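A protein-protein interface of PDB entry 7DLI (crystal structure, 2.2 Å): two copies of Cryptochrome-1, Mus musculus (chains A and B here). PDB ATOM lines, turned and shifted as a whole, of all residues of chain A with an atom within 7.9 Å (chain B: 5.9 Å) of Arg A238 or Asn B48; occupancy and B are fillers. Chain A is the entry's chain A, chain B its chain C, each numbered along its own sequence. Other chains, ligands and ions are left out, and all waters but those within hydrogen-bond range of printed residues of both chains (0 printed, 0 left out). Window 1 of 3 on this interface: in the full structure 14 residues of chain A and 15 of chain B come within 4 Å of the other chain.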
ATOM      1  N   LYS A 230     -17.046  20.747  10.790  1.00  0.00           N
ATOM      2  CA  LYS A 230     -17.973  20.575  11.912  1.00  0.00           C
ATOM      3  C   LYS A 230     -19.261  19.862  11.495  1.00  0.00           C
ATOM      4  O   LYS A 230     -19.733  18.967  12.203  1.00  0.00           O
ATOM      5  CB  LYS A 230     -18.313  21.930  12.539  1.00  0.00           C
ATOM      6  N   VAL A 233     -17.767  16.287   9.039  1.00  0.00           N
ATOM      7  CA  VAL A 233     -16.700  15.507   9.662  1.00  0.00           C
ATOM      8  C   VAL A 233     -16.880  15.358  11.170  1.00  0.00           C
ATOM      9  O   VAL A 233     -16.032  14.741  11.831  1.00  0.00           O
ATOM     10  CB  VAL A 233     -15.306  16.110   9.367  1.00  0.00           C
ATOM     11  N   ALA A 234     -17.956  15.896  11.739  1.00  0.00           N
ATOM     12  CA  ALA A 234     -18.208  15.719  13.164  1.00  0.00           C
ATOM     13  C   ALA A 234     -19.652  15.379  13.497  1.00  0.00           C
ATOM     14  O   ALA A 234     -19.935  15.078  14.663  1.00  0.00           O
ATOM     15  CB  ALA A 234     -17.805  16.983  13.945  1.00  0.00           C
ATOM     16  N   ASN A 235     -20.564  15.384  12.521  1.00  0.00           N
ATOM     17  CA  ASN A 235     -22.004  15.313  12.777  1.00  0.00           C
ATOM     18  C   ASN A 235     -22.434  16.312  13.850  1.00  0.00           C
ATOM     19  O   ASN A 235     -23.325  16.043  14.663  1.00  0.00           O
ATOM     20  CB  ASN A 235     -22.449  13.899  13.146  1.00  0.00           C
ATOM     21  CG  ASN A 235     -23.917  13.697  12.888  1.00  0.00           C
ATOM     22  OD1 ASN A 235     -24.464  14.304  11.966  1.00  0.00           O
ATOM     23  ND2 ASN A 235     -24.570  12.852  13.686  1.00  0.00           N
ATOM     24  N   PHE A 236     -21.787  17.476  13.842  1.00  0.00           N
ATOM     25  CA  PHE A 236     -22.043  18.587  14.750  1.00  0.00           C
ATOM     26  C   PHE A 236     -21.703  18.244  16.192  1.00  0.00           C
ATOM     27  O   PHE A 236     -22.112  18.959  17.113  1.00  0.00           O
ATOM     28  CB  PHE A 236     -23.490  19.086  14.641  1.00  0.00           C
ATOM     29  CG  PHE A 236     -23.868  19.567  13.265  1.00  0.00           C
ATOM     30  CD1 PHE A 236     -23.556  20.862  12.850  1.00  0.00           C
ATOM     31  CD2 PHE A 236     -24.548  18.732  12.383  1.00  0.00           C
ATOM     32  CE1 PHE A 236     -23.907  21.322  11.588  1.00  0.00           C
ATOM     33  CE2 PHE A 236     -24.912  19.183  11.113  1.00  0.00           C
ATOM     34  CZ  PHE A 236     -24.580  20.482  10.715  1.00  0.00           C
ATOM     35  N   GLU A 237     -20.942  17.173  16.406  1.00  0.00           N
ATOM     36  CA  GLU A 237     -20.423  16.806  17.719  1.00  0.00           C
ATOM     37  C   GLU A 237     -18.985  17.312  17.896  1.00  0.00           C
ATOM     38  O   GLU A 237     -18.354  17.816  16.966  1.00  0.00           O
ATOM     39  CB  GLU A 237     -20.493  15.282  17.911  1.00  0.00           C
ATOM     40  N   ARG A 238     -18.480  17.192  19.114  1.00  0.00           N
ATOM     41  CA  ARG A 238     -17.071  17.442  19.368  1.00  0.00           C
ATOM     42  C   ARG A 238     -16.284  16.175  19.075  1.00  0.00           C
ATOM     43  O   ARG A 238     -16.601  15.122  19.648  1.00  0.00           O
ATOM     44  CB  ARG A 238     -16.849  17.892  20.791  1.00  0.00           C
ATOM     45  N   PRO A 239     -15.330  16.188  18.146  1.00  0.00           N
ATOM     46  CA  PRO A 239     -14.549  14.963  17.881  1.00  0.00           C
ATOM     47  C   PRO A 239     -13.482  14.717  18.942  1.00  0.00           C
ATOM     48  O   PRO A 239     -13.128  15.606  19.720  1.00  0.00           O
ATOM     49  CB  PRO A 239     -13.839  15.222  16.526  1.00  0.00           C
ATOM     50  CG  PRO A 239     -14.423  16.482  15.999  1.00  0.00           C
ATOM     51  CD  PRO A 239     -15.297  17.109  17.040  1.00  0.00           C
ATOM     52  N   ARG A 240     -12.977  13.491  18.955  1.00  0.00           N
ATOM     53  CA  ARG A 240     -11.915  13.115  19.889  1.00  0.00           C
ATOM     54  C   ARG A 240     -10.613  13.865  19.569  1.00  0.00           C
ATOM     55  O   ARG A 240     -10.365  14.258  18.424  1.00  0.00           O
ATOM     56  CB  ARG A 240     -11.712  11.597  19.848  1.00  0.00           C
ATOM     57  N   MET A 241      -9.804  14.081  20.603  1.00  0.00           N
ATOM     58  CA  MET A 241      -8.487  14.661  20.450  1.00  0.00           C
ATOM     59  C   MET A 241      -7.515  13.618  19.922  1.00  0.00           C
ATOM     60  O   MET A 241      -7.604  12.437  20.257  1.00  0.00           O
ATOM     61  CB  MET A 241      -7.970  15.211  21.782  1.00  0.00           C
ATOM     62  N   SER A 287     -25.511  23.671  22.828  1.00  0.00           N
ATOM     63  CA  SER A 287     -24.146  23.163  22.821  1.00  0.00           C
ATOM     64  C   SER A 287     -23.471  23.373  21.470  1.00  0.00           C
ATOM     65  O   SER A 287     -22.241  23.439  21.403  1.00  0.00           O
ATOM     66  CB  SER A 287     -24.135  21.688  23.224  1.00  0.00           C
ATOM     67  OG  SER A 287     -24.915  20.927  22.338  1.00  0.00           O
ATOM     68  N   SER B  46     -12.944   7.970  15.808  1.00  0.00           N
ATOM     69  CA  SER B  46     -12.808   9.399  16.057  1.00  0.00           C
ATOM     70  C   SER B  46     -13.980   9.996  16.839  1.00  0.00           C
ATOM     71  O   SER B  46     -13.912  11.172  17.219  1.00  0.00           O
ATOM     72  CB  SER B  46     -12.635  10.143  14.725  1.00  0.00           C
ATOM     73  OG  SER B  46     -13.760   9.960  13.882  1.00  0.00           O
ATOM     74  N   SER B  47     -15.028   9.218  17.119  1.00  0.00           N
ATOM     75  CA  SER B  47     -16.251   9.756  17.709  1.00  0.00           C
ATOM     76  C   SER B  47     -16.133   9.895  19.222  1.00  0.00           C
ATOM     77  O   SER B  47     -15.373   9.184  19.887  1.00  0.00           O
ATOM     78  CB  SER B  47     -17.455   8.864  17.380  1.00  0.00           C
ATOM     79  N   ASN B  48     -16.927  10.816  19.761  1.00  0.00           N
ATOM     80  CA  ASN B  48     -16.984  11.118  21.182  1.00  0.00           C
ATOM     81  C   ASN B  48     -18.227  10.535  21.853  1.00  0.00           C
ATOM     82  O   ASN B  48     -18.497  10.858  23.012  1.00  0.00           O
ATOM     83  CB  ASN B  48     -16.977  12.639  21.378  1.00  0.00           C
ATOM     84  CG  ASN B  48     -16.116  13.088  22.540  1.00  0.00           C
ATOM     85  OD1 ASN B  48     -15.185  12.394  22.940  1.00  0.00           O
ATOM     86  ND2 ASN B  48     -16.454  14.244  23.118  1.00  0.00           N
ATOM     87  N   VAL B  49     -18.992   9.688  21.154  1.00  0.00           N
ATOM     88  CA  VAL B  49     -20.382   9.445  21.551  1.00  0.00           C
ATOM     89  C   VAL B  49     -20.490   8.579  22.808  1.00  0.00           C
ATOM     90  O   VAL B  49     -21.472   8.694  23.554  1.00  0.00           O
ATOM     91  CB  VAL B  49     -21.180   8.828  20.383  1.00  0.00           C
ATOM     92  N   GLY B  50     -19.523   7.690  23.058  1.00  0.00           N
ATOM     93  CA  GLY B  50     -19.582   6.833  24.228  1.00  0.00           C
ATOM     94  C   GLY B  50     -19.021   7.455  25.497  1.00  0.00           C
ATOM     95  O   GLY B  50     -18.661   6.727  26.426  1.00  0.00           O
ATOM     96  N   ILE B  51     -18.951   8.793  25.556  1.00  0.00           N
ATOM     97  CA  ILE B  51     -18.291   9.474  26.673  1.00  0.00           C
ATOM     98  C   ILE B  51     -18.983   9.193  28.012  1.00  0.00           C
ATOM     99  O   ILE B  51     -18.325   9.118  29.056  1.00  0.00           O
ATOM    100  CB  ILE B  51     -18.167  10.987  26.394  1.00  0.00           C
ATOM    101  CG1 ILE B  51     -17.178  11.625  27.375  1.00  0.00           C
ATOM    102  CG2 ILE B  51     -19.529  11.691  26.455  1.00  0.00           C
ATOM    103  CD1 ILE B  51     -16.840  13.120  27.059  1.00  0.00           C
ATOM    104  N   ASN B  52     -20.312   9.083  28.026  1.00  0.00           N
ATOM    105  CA  ASN B  52     -20.986   8.897  29.311  1.00  0.00           C
ATOM    106  C   ASN B  52     -20.625   7.546  29.939  1.00  0.00           C
ATOM    107  O   ASN B  52     -20.369   7.457  31.149  1.00  0.00           O
ATOM    108  CB  ASN B  52     -22.492   9.045  29.119  1.00  0.00           C
ATOM    109  CG  ASN B  52     -22.934  10.500  29.116  1.00  0.00           C
ATOM    110  OD1 ASN B  52     -22.190  11.400  29.552  1.00  0.00           O
ATOM    111  ND2 ASN B  52     -24.140  10.748  28.613  1.00  0.00           N
ATOM    112  N   GLY B 201      -8.248  11.278  25.454  1.00  0.00           N
ATOM    113  CA  GLY B 201      -8.573  11.902  24.189  1.00  0.00           C
ATOM    114  C   GLY B 201     -10.011  12.332  23.989  1.00  0.00           C
ATOM    115  O   GLY B 201     -10.371  12.713  22.873  1.00  0.00           O
ATOM    116  N   PHE B 202     -10.856  12.246  25.002  1.00  0.00           N
ATOM    117  CA  PHE B 202     -12.227  12.712  24.856  1.00  0.00           C
ATOM    118  C   PHE B 202     -12.277  14.222  25.026  1.00  0.00           C
ATOM    119  O   PHE B 202     -11.586  14.786  25.878  1.00  0.00           O
ATOM    120  CB  PHE B 202     -13.147  12.037  25.880  1.00  0.00           C
ATOM    121  CG  PHE B 202     -13.441  10.596  25.579  1.00  0.00           C
ATOM    122  CD1 PHE B 202     -14.496  10.247  24.753  1.00  0.00           C
ATOM    123  CD2 PHE B 202     -12.668   9.587  26.131  1.00  0.00           C
ATOM    124  CE1 PHE B 202     -14.782   8.917  24.472  1.00  0.00           C
ATOM    125  CE2 PHE B 202     -12.946   8.235  25.852  1.00  0.00           C
ATOM    126  CZ  PHE B 202     -14.004   7.910  25.012  1.00  0.00           C
ATOM    127  N   ASP B 203     -13.092  14.876  24.209  1.00  0.00           N
ATOM    128  CA  ASP B 203     -13.375  16.295  24.399  1.00  0.00           C
ATOM    129  C   ASP B 203     -14.471  16.420  25.456  1.00  0.00           C
ATOM    130  O   ASP B 203     -15.585  15.918  25.265  1.00  0.00           O
ATOM    131  CB  ASP B 203     -13.791  16.958  23.086  1.00  0.00           C
ATOM    132  N   THR B 204     -14.144  17.058  26.580  1.00  0.00           N
ATOM    133  CA  THR B 204     -15.015  17.135  27.746  1.00  0.00           C
ATOM    134  C   THR B 204     -15.775  18.454  27.854  1.00  0.00           C
ATOM    135  O   THR B 204     -16.390  18.709  28.892  1.00  0.00           O
ATOM    136  CB  THR B 204     -14.204  16.918  29.025  1.00  0.00           C
ATOM    137  OG1 THR B 204     -13.154  17.886  29.083  1.00  0.00           O
ATOM    138  CG2 THR B 204     -13.601  15.517  29.046  1.00  0.00           C
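The backbone NH (N) of Met A241 lies within hydrogen-bond range of the backbone carbonyl oxygen (O) of Gly B201, 2.7 Å away. The backbone carbonyl oxygen (O) of Ser B46 sits at hydrogen-bond distance from the backbone NH (N) of Arg A240 (3.0 Å).
The side-chain amide nitrogen of Asn B48 sits at hydrogen-bond distance from the backbone carbonyl oxygen of Asp B203 (2.9 Å).
Among the printed residues, pairs that only touch across the chains: Arg A238 with Asn B48, Arg A240 with Gly B201, Pro A239 with Asp B203, Pro A239 with Ser B46 and Arg A238 with Asp B203.
Arg A238 touches two residues of chain B. No residue of chain A comes within 4 Å of Ser B47. Val B49 touches none of the printed residues of chain A. Printed residues of chain A within 4 Å of Asp B203: Arg A238 and Pro A239. Printed residues of chain B within 4 Å of Met A241: Gly B201 (2.7 Å). Printed residues of chain B within 4 Å of Arg A240: Ser B46 (3.0 Å) and Gly B201 (3.4 Å). Val A233 touches none of the printed residues of chain B. Ser A287 touches none of the printed residues of chain B. The nearest residue of chain A that does not touch Asn B48 is Arg A240 (4.5 Å). The nearest printed residue of chain B that does not touch Arg A240 is Ser B47 (4.4 Å).
Of the 11 printed residues of chain B, 4 touch a printed residue of chain A. Printed residues of chain B that touch a printed residue of chain A: Ser B46, Asn B48, Gly B201 and Asp B203. Of the 11 printed residues of chain A, 4 touch a printed residue of chain B. Printed residues of chain A that touch a printed residue of chain B: Arg A238, Pro A239, Arg A240 and Met A241. Hydrophobic or aromatic side chains of chain A within 4 Å of the printed part of chain B: Met A241. Among the printed residues, no Asp or Glu carboxylate lies within 4 Å of a Lys or Arg side-chain nitrogen of the other chain.
No position is printed for both chains.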
